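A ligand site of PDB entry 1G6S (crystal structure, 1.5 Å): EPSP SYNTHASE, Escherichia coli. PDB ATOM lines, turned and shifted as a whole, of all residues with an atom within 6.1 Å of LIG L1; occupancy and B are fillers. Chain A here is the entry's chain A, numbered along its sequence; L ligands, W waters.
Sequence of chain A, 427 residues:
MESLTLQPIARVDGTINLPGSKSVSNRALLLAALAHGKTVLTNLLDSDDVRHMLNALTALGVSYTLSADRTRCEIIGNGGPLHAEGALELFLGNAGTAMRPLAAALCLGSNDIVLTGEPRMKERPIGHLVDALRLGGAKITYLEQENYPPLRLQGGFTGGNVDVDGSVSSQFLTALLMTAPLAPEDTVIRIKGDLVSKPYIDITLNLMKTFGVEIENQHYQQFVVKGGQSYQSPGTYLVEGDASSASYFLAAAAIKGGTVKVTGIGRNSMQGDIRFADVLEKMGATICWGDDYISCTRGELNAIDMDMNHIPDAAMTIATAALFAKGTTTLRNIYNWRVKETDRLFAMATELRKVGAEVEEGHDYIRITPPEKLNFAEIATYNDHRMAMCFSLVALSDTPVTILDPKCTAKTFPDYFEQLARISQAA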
ATOM      1  N   LYS A  22      19.492   3.420  22.824  1.00  0.00           N
ATOM      2  CA  LYS A  22      20.937   3.170  22.743  1.00  0.00           C
ATOM      3  C   LYS A  22      21.380   2.944  21.278  1.00  0.00           C
ATOM      4  O   LYS A  22      22.431   3.482  20.849  1.00  0.00           O
ATOM      5  CB  LYS A  22      21.283   1.942  23.609  1.00  0.00           C
ATOM      6  CG  LYS A  22      22.766   1.473  23.502  1.00  0.00           C
ATOM      7  CD  LYS A  22      22.858   0.081  22.825  1.00  0.00           C
ATOM      8  CE  LYS A  22      22.485  -1.034  23.829  1.00  0.00           C
ATOM      9  NZ  LYS A  22      22.338  -2.341  23.118  1.00  0.00           N
ATOM     10  N   ASP A  49      26.961   2.677  27.591  1.00  0.00           N
ATOM     11  CA  ASP A  49      27.323   2.423  26.204  1.00  0.00           C
ATOM     12  C   ASP A  49      27.472   3.711  25.408  1.00  0.00           C
ATOM     13  O   ASP A  49      28.330   3.762  24.524  1.00  0.00           O
ATOM     14  CB  ASP A  49      26.275   1.524  25.510  1.00  0.00           C
ATOM     15  CG  ASP A  49      26.411   0.059  25.913  1.00  0.00           C
ATOM     16  OD1 ASP A  49      27.331  -0.320  26.667  1.00  0.00           O
ATOM     17  OD2 ASP A  49      25.571  -0.702  25.392  1.00  0.00           O
ATOM     18  N   ASN A  94      31.554  -2.531  27.428  1.00  0.00           N
ATOM     19  CA  ASN A  94      31.050  -3.763  26.787  1.00  0.00           C
ATOM     20  C   ASN A  94      30.004  -3.329  25.773  1.00  0.00           C
ATOM     21  O   ASN A  94      28.986  -3.998  25.565  1.00  0.00           O
ATOM     22  CB  ASN A  94      30.401  -4.715  27.791  1.00  0.00           C
ATOM     23  CG  ASN A  94      30.214  -6.121  27.234  1.00  0.00           C
ATOM     24  OD1 ASN A  94      30.776  -6.486  26.189  1.00  0.00           O
ATOM     25  ND2 ASN A  94      29.434  -6.938  27.954  1.00  0.00           N
ATOM     26  N   ALA A  95      30.284  -2.197  25.132  1.00  0.00           N
ATOM     27  CA  ALA A  95      29.352  -1.638  24.156  1.00  0.00           C
ATOM     28  C   ALA A  95      29.561  -2.150  22.750  1.00  0.00           C
ATOM     29  O   ALA A  95      30.451  -1.660  22.029  1.00  0.00           O
ATOM     30  CB  ALA A  95      29.465  -0.093  24.173  1.00  0.00           C
ATOM     31  N   GLY A  96      28.757  -3.125  22.318  1.00  0.00           N
ATOM     32  CA  GLY A  96      28.911  -3.610  20.953  1.00  0.00           C
ATOM     33  C   GLY A  96      28.626  -2.508  19.938  1.00  0.00           C
ATOM     34  O   GLY A  96      29.264  -2.482  18.865  1.00  0.00           O
ATOM     35  N   THR A  97      27.697  -1.620  20.250  1.00  0.00           N
ATOM     36  CA  THR A  97      27.337  -0.549  19.301  1.00  0.00           C
ATOM     37  C   THR A  97      28.396   0.501  19.185  1.00  0.00           C
ATOM     38  O   THR A  97      28.269   1.404  18.335  1.00  0.00           O
ATOM     39  CB  THR A  97      25.962   0.081  19.595  1.00  0.00           C
ATOM     40  OG1 THR A  97      25.991   0.673  20.900  1.00  0.00           O
ATOM     41  CG2 THR A  97      24.842  -0.966  19.487  1.00  0.00           C
ATOM     42  N   ARG A 100      31.756  -2.566  17.450  1.00  0.00           N
ATOM     43  CA  ARG A 100      31.656  -3.039  16.079  1.00  0.00           C
ATOM     44  C   ARG A 100      31.698  -1.877  15.068  1.00  0.00           C
ATOM     45  O   ARG A 100      32.517  -1.887  14.144  1.00  0.00           O
ATOM     46  CB  ARG A 100      30.391  -3.913  15.918  1.00  0.00           C
ATOM     47  CG  ARG A 100      30.592  -5.385  16.359  1.00  0.00           C
ATOM     48  CD  ARG A 100      30.758  -5.525  17.904  1.00  0.00           C
ATOM     49  NE  ARG A 100      30.828  -6.921  18.321  1.00  0.00           N
ATOM     50  CZ  ARG A 100      29.765  -7.660  18.699  1.00  0.00           C
ATOM     51  NH1 ARG A 100      29.922  -8.922  19.079  1.00  0.00           N
ATOM     52  NH2 ARG A 100      28.548  -7.132  18.704  1.00  0.00           N
ATOM     53  N   MET A 121      33.946  -8.173  26.991  1.00  0.00           N
ATOM     54  CA  MET A 121      34.033  -7.764  25.587  1.00  0.00           C
ATOM     55  C   MET A 121      35.132  -8.503  24.850  1.00  0.00           C
ATOM     56  O   MET A 121      35.019  -8.750  23.634  1.00  0.00           O
ATOM     57  CB  MET A 121      34.255  -6.237  25.491  1.00  0.00           C
ATOM     58  CG  MET A 121      34.436  -5.712  24.056  1.00  0.00           C
ATOM     59  SD  MET A 121      33.099  -6.149  22.862  1.00  0.00           S
ATOM     60  CE  MET A 121      31.818  -4.881  23.309  1.00  0.00           C
ATOM     61  N   ARG A 124      33.548 -11.553  23.358  1.00  0.00           N
ATOM     62  CA  ARG A 124      32.414 -11.396  22.426  1.00  0.00           C
ATOM     63  C   ARG A 124      33.020 -11.381  21.020  1.00  0.00           C
ATOM     64  O   ARG A 124      33.911 -10.571  20.719  1.00  0.00           O
ATOM     65  CB  ARG A 124      31.625 -10.143  22.759  1.00  0.00           C
ATOM     66  CG  ARG A 124      30.870 -10.295  24.097  1.00  0.00           C
ATOM     67  CD  ARG A 124      30.020  -9.070  24.383  1.00  0.00           C
ATOM     68  NE  ARG A 124      28.986  -8.936  23.367  1.00  0.00           N
ATOM     69  CZ  ARG A 124      28.340  -7.801  23.109  1.00  0.00           C
ATOM     70  NH1 ARG A 124      27.415  -7.774  22.151  1.00  0.00           N
ATOM     71  NH2 ARG A 124      28.554  -6.700  23.836  1.00  0.00           N
ATOM     72  N   GLN A 171      25.448  -6.630  13.731  1.00  0.00           N
ATOM     73  CA  GLN A 171      26.303  -5.473  13.906  1.00  0.00           C
ATOM     74  C   GLN A 171      27.492  -5.444  12.970  1.00  0.00           C
ATOM     75  O   GLN A 171      28.000  -4.359  12.664  1.00  0.00           O
ATOM     76  CB  GLN A 171      26.782  -5.380  15.343  1.00  0.00           C
ATOM     77  CG  GLN A 171      25.651  -5.004  16.311  1.00  0.00           C
ATOM     78  CD  GLN A 171      26.163  -4.786  17.711  1.00  0.00           C
ATOM     79  OE1 GLN A 171      27.374  -4.682  17.954  1.00  0.00           O
ATOM     80  NE2 GLN A 171      25.231  -4.663  18.668  1.00  0.00           N
ATOM     81  N   ASP A 313      16.480  -8.771  22.191  1.00  0.00           N
ATOM     82  CA  ASP A 313      16.695  -8.076  23.484  1.00  0.00           C
ATOM     83  C   ASP A 313      15.395  -8.002  24.284  1.00  0.00           C
ATOM     84  O   ASP A 313      15.343  -8.447  25.436  1.00  0.00           O
ATOM     85  CB  ASP A 313      17.255  -6.675  23.254  1.00  0.00           C
ATOM     86  CG  ASP A 313      18.661  -6.666  22.645  1.00  0.00           C
ATOM     87  OD1 ASP A 313      19.126  -5.558  22.356  1.00  0.00           O
ATOM     88  OD2 ASP A 313      19.268  -7.730  22.452  1.00  0.00           O
ATOM     89  N   MET A 316      13.909 -11.182  26.129  1.00  0.00           N
ATOM     90  CA  MET A 316      14.277 -11.584  27.492  1.00  0.00           C
ATOM     91  C   MET A 316      13.154 -11.206  28.456  1.00  0.00           C
ATOM     92  O   MET A 316      12.899 -11.913  29.433  1.00  0.00           O
ATOM     93  CB  MET A 316      15.570 -10.899  27.931  1.00  0.00           C
ATOM     94  CG  MET A 316      16.794 -11.280  27.106  1.00  0.00           C
ATOM     95  SD  MET A 316      18.245 -10.387  27.715  1.00  0.00           S
ATOM     96  CE  MET A 316      18.498 -11.057  29.422  1.00  0.00           C
ATOM     97  N   LYS A 340      26.276 -12.224  24.031  1.00  0.00           N
ATOM     98  CA  LYS A 340      26.019 -10.834  24.384  1.00  0.00           C
ATOM     99  C   LYS A 340      26.602 -10.441  25.757  1.00  0.00           C
ATOM    100  O   LYS A 340      27.697 -10.910  26.070  1.00  0.00           O
ATOM    101  CB  LYS A 340      24.531 -10.542  24.204  1.00  0.00           C
ATOM    102  CG  LYS A 340      24.287 -10.425  22.652  1.00  0.00           C
ATOM    103  CD  LYS A 340      22.826 -10.320  22.318  1.00  0.00           C
ATOM    104  CE  LYS A 340      22.722  -9.974  20.815  1.00  0.00           C
ATOM    105  NZ  LYS A 340      21.306 -10.051  20.319  1.00  0.00           N
ATOM    106  N   GLU A 341      25.919  -9.626  26.574  1.00  0.00           N
ATOM    107  CA  GLU A 341      26.521  -9.181  27.845  1.00  0.00           C
ATOM    108  C   GLU A 341      26.963 -10.314  28.747  1.00  0.00           C
ATOM    109  O   GLU A 341      27.923 -10.157  29.512  1.00  0.00           O
ATOM    110  CB  GLU A 341      25.594  -8.222  28.601  1.00  0.00           C
ATOM    111  CG  GLU A 341      25.531  -6.814  27.942  1.00  0.00           C
ATOM    112  CD  GLU A 341      24.599  -6.678  26.712  1.00  0.00           C
ATOM    113  OE1 GLU A 341      24.271  -7.686  26.029  1.00  0.00           O
ATOM    114  OE2 GLU A 341      24.243  -5.511  26.415  1.00  0.00           O
ATOM    115  N   ARG A 344      23.216 -15.366  27.865  1.00  0.00           N
ATOM    116  CA  ARG A 344      21.869 -15.169  28.414  1.00  0.00           C
ATOM    117  C   ARG A 344      21.003 -16.414  28.459  1.00  0.00           C
ATOM    118  O   ARG A 344      20.070 -16.455  29.261  1.00  0.00           O
ATOM    119  CB  ARG A 344      21.167 -14.015  27.642  1.00  0.00           C
ATOM    120  CG  ARG A 344      21.827 -12.681  27.968  1.00  0.00           C
ATOM    121  CD  ARG A 344      21.464 -11.638  26.904  1.00  0.00           C
ATOM    122  NE  ARG A 344      21.613 -10.306  27.487  1.00  0.00           N
ATOM    123  CZ  ARG A 344      21.273  -9.184  26.867  1.00  0.00           C
ATOM    124  NH1 ARG A 344      21.390  -8.019  27.494  1.00  0.00           N
ATOM    125  NH2 ARG A 344      20.888  -9.192  25.577  1.00  0.00           N
ATOM    126  N   ASP A 384      24.940  -7.803  33.454  1.00  0.00           N
ATOM    127  CA  ASP A 384      23.978  -7.656  32.359  1.00  0.00           C
ATOM    128  C   ASP A 384      22.749  -6.861  32.778  1.00  0.00           C
ATOM    129  O   ASP A 384      21.855  -7.377  33.455  1.00  0.00           O
ATOM    130  CB  ASP A 384      23.584  -9.048  31.848  1.00  0.00           C
ATOM    131  CG  ASP A 384      22.632  -9.010  30.649  1.00  0.00           C
ATOM    132  OD1 ASP A 384      22.216  -7.917  30.234  1.00  0.00           O
ATOM    133  OD2 ASP A 384      22.301 -10.099  30.134  1.00  0.00           O
ATOM    134  N   HIS A 385      22.711  -5.597  32.365  1.00  0.00           N
ATOM    135  CA  HIS A 385      21.563  -4.712  32.619  1.00  0.00           C
ATOM    136  C   HIS A 385      20.195  -5.422  32.464  1.00  0.00           C
ATOM    137  O   HIS A 385      19.311  -5.220  33.297  1.00  0.00           O
ATOM    138  CB  HIS A 385      21.603  -3.485  31.636  1.00  0.00           C
ATOM    139  CG  HIS A 385      21.701  -3.835  30.169  1.00  0.00           C
ATOM    140  ND1 HIS A 385      21.016  -3.123  29.194  1.00  0.00           N
ATOM    141  CD2 HIS A 385      22.445  -4.757  29.498  1.00  0.00           C
ATOM    142  CE1 HIS A 385      21.326  -3.592  27.999  1.00  0.00           C
ATOM    143  NE2 HIS A 385      22.184  -4.590  28.149  1.00  0.00           N
ATOM    144  N   ARG A 386      20.051  -6.254  31.420  1.00  0.00           N
ATOM    145  CA  ARG A 386      18.731  -6.839  31.212  1.00  0.00           C
ATOM    146  C   ARG A 386      18.414  -7.960  32.164  1.00  0.00           C
ATOM    147  O   ARG A 386      17.228  -8.226  32.420  1.00  0.00           O
ATOM    148  CB  ARG A 386      18.522  -7.290  29.766  1.00  0.00           C
ATOM    149  CG  ARG A 386      18.581  -6.087  28.787  1.00  0.00           C
ATOM    150  CD  ARG A 386      17.833  -6.402  27.438  1.00  0.00           C
ATOM    151  NE  ARG A 386      18.268  -5.373  26.475  1.00  0.00           N
ATOM    152  CZ  ARG A 386      17.955  -4.079  26.544  1.00  0.00           C
ATOM    153  NH1 ARG A 386      18.558  -3.246  25.672  1.00  0.00           N
ATOM    154  NH2 ARG A 386      16.983  -3.618  27.343  1.00  0.00           N
ATOM    155  N   LYS A 411      24.155   0.224  31.914  1.00  0.00           N
ATOM    156  CA  LYS A 411      24.633   0.027  30.563  1.00  0.00           C
ATOM    157  C   LYS A 411      23.706   0.733  29.550  1.00  0.00           C
ATOM    158  O   LYS A 411      24.203   1.335  28.582  1.00  0.00           O
ATOM    159  CB  LYS A 411      24.758  -1.468  30.214  1.00  0.00           C
ATOM    160  CG  LYS A 411      25.553  -1.687  28.898  1.00  0.00           C
ATOM    161  CD  LYS A 411      25.899  -3.173  28.686  1.00  0.00           C
ATOM    162  CE  LYS A 411      26.813  -3.405  27.496  1.00  0.00           C
ATOM    163  NZ  LYS A 411      26.069  -3.354  26.192  1.00  0.00           N
ATOM    164  N   THR A 412      22.391   0.661  29.796  1.00  0.00           N
ATOM    165  CA  THR A 412      21.414   1.307  28.935  1.00  0.00           C
ATOM    166  C   THR A 412      20.345   2.102  29.669  1.00  0.00           C
ATOM    167  O   THR A 412      19.618   2.852  29.029  1.00  0.00           O
ATOM    168  CB  THR A 412      20.622   0.285  28.077  1.00  0.00           C
ATOM    169  OG1 THR A 412      19.907  -0.603  28.947  1.00  0.00           O
ATOM    170  CG2 THR A 412      21.558  -0.472  27.106  1.00  0.00           C
HETATM  171  P1  LIG L   1      25.623  -4.789  22.479  1.00  0.00           P
HETATM  172  O1  LIG L   1      24.806  -3.588  22.252  1.00  0.00           O
HETATM  173  O2  LIG L   1      26.244  -5.341  21.279  1.00  0.00           O
HETATM  174  O3  LIG L   1      26.664  -4.576  23.584  1.00  0.00           O
HETATM  175  O4  LIG L   1      21.263  -4.473  24.792  1.00  0.00           O
HETATM  176  O5  LIG L   1      20.306  -6.434  25.223  1.00  0.00           O
HETATM  177  C1  LIG L   1      24.575  -6.105  22.963  1.00  0.00           C
HETATM  178  C2  LIG L   1      22.329  -6.519  24.083  1.00  0.00           C
HETATM  179  C3  LIG L   1      21.209  -5.750  24.767  1.00  0.00           C
HETATM  180  N1  LIG L   1      23.416  -5.570  23.667  1.00  0.00           N
HETATM  181  C1  LG2 L   2      21.972  -3.767  18.124  1.00  0.00           C
HETATM  182  C2  LG2 L   2      21.849  -5.018  17.516  1.00  0.00           C
HETATM  183  C3  LG2 L   2      21.600  -6.272  18.332  1.00  0.00           C
HETATM  184  C4  LG2 L   2      21.134  -5.964  19.765  1.00  0.00           C
HETATM  185  C5  LG2 L   2      22.000  -4.868  20.386  1.00  0.00           C
HETATM  186  C6  LG2 L   2      21.804  -3.594  19.548  1.00  0.00           C
HETATM  187  C7  LG2 L   2      22.219  -2.581  17.247  1.00  0.00           C
HETATM  188  O1  LG2 L   2      22.802  -7.141  18.295  1.00  0.00           O
HETATM  189  O2  LG2 L   2      21.169  -7.179  20.530  1.00  0.00           O
HETATM  190  O3  LG2 L   2      21.589  -4.623  21.736  1.00  0.00           O
HETATM  191  O4  LG2 L   2      22.707  -2.782  16.105  1.00  0.00           O
HETATM  192  O5  LG2 L   2      21.908  -1.483  17.701  1.00  0.00           O
HETATM  193  P1  LG2 L   2      22.907  -8.485  17.311  1.00  0.00           P
HETATM  194  O6  LG2 L   2      22.789  -8.020  15.909  1.00  0.00           O
HETATM  195  O7  LG2 L   2      21.750  -9.352  17.785  1.00  0.00           O
HETATM  196  O8  LG2 L   2      24.265  -9.037  17.639  1.00  0.00           O
HETATM  197  O   HOH W   1      26.060  -1.313  22.718  1.00  0.00           O
HETATM  198  O   HOH W   2      25.820  -7.805  19.681  1.00  0.00           O
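The backbone carbonyl oxygen of Asn 94 lies close to an oxygen (O3) of LIG L1 (3.1 Å). An oxygen (O5) of LIG L1 sits close to the side-chain carboxylate (OD1) of Asp 313, 3.2 Å away. Residues that only touch LIG L1: Thr 97 and Ala 95. Hydrophobic or aromatic side chains within 4 Å of LIG L1: His 385. 14 residues have an atom within 4 Å of LIG L1: Lys 22, Asn 94, Ala 95, Gly 96, Thr 97, Arg 100, Arg 124, Gln 171, Asp 313, Glu 341, Arg 344, His 385, Arg 386 and Lys 411. The nearest printed residue that does not touch LIG L1 is Lys 340 (4.2 Å).
An oxygen (O3) of LG2 L2 sits at hydrogen-bond distance from a nitrogen (N1) of LIG L1, at 2.8 Å.
NH2 of Arg 344 lies within salt-bridge range of OD2 of Asp 313 (3.8 Å). NE of Arg 344 sits close to SD of Met 316 (3.4 Å). OD2 of Asp 384 is in salt-bridge range of NE of Arg 344 (2.7 Å). The backbone carbonyl oxygen (O) of Gly 96 lies close to the side-chain amide oxygen (OE1) of Gln 171 (3.0 Å). OE2 of Glu 341 is in salt-bridge range of NZ of Lys 411, 2.8 Å away. OE2 of Glu 341 lies within hydrogen-bond range of NE2 of His 385. The side-chain amino group (NZ) of Lys 411 sits close to the backbone carbonyl oxygen (O) of Asn 94 (3.1 Å). OD2 of Asp 313 lies within salt-bridge range of NZ of Lys 340 (3.8 Å).
Water W1 lies within hydrogen-bond range of an oxygen (O1) of LIG L1, the side-chain hydroxyl (OG1) of Thr 97, the side-chain carboxylate (OD2) of Asp 49 and the backbone NH (N) of Gly 96.
An oxygen (O5) of LIG L1 lies within salt-bridge range of the guanidinium group (NE) of Arg 386 (2.6 Å). An oxygen (O2) of LIG L1 lies within salt-bridge range of the guanidinium group (NH1) of Arg 124 (2.8 Å). An oxygen (O5) of LIG L1 is in salt-bridge range of the guanidinium group (NH2) of Arg 344 (2.8 Å). The backbone NH of Gly 96 lies within hydrogen-bond range of an oxygen (O3) of LIG L1 (2.8 Å). The side-chain carboxylate of Glu 341 is in salt-bridge range of a nitrogen (N1) of LIG L1. The side-chain amide nitrogen of Gln 171 is in hydrogen-bond range of an oxygen (O2) of LIG L1. NZ of Lys 22 is in salt-bridge range of O1 of LIG L1, at 2.9 Å. The side-chain amino group (NZ) of Lys 411 is in salt-bridge range of an oxygen (O3) of LIG L1 (2.9 Å). An oxygen (O4) of LIG L1 lies close to a ring nitrogen (NE2) of His 385. The guanidinium group of Arg 100 is in salt-bridge range of an oxygen (O2) of LIG L1. An oxygen (O1) of LG2 L2 sits close to the side-chain amide nitrogen (NE2) of Gln 171, at 3.5 Å. An oxygen (O3) of LG2 L2 sits at hydrogen-bond distance from the side-chain amino group (NZ) of Lys 22, 2.8 Å away. The side-chain carboxylate (OD1) of Asp 313 sits at hydrogen-bond distance from an oxygen (O3) of LG2 L2 (2.7 Å). An oxygen (O7) of LG2 L2 lies within salt-bridge range of the side-chain amino group (NZ) of Lys 340.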
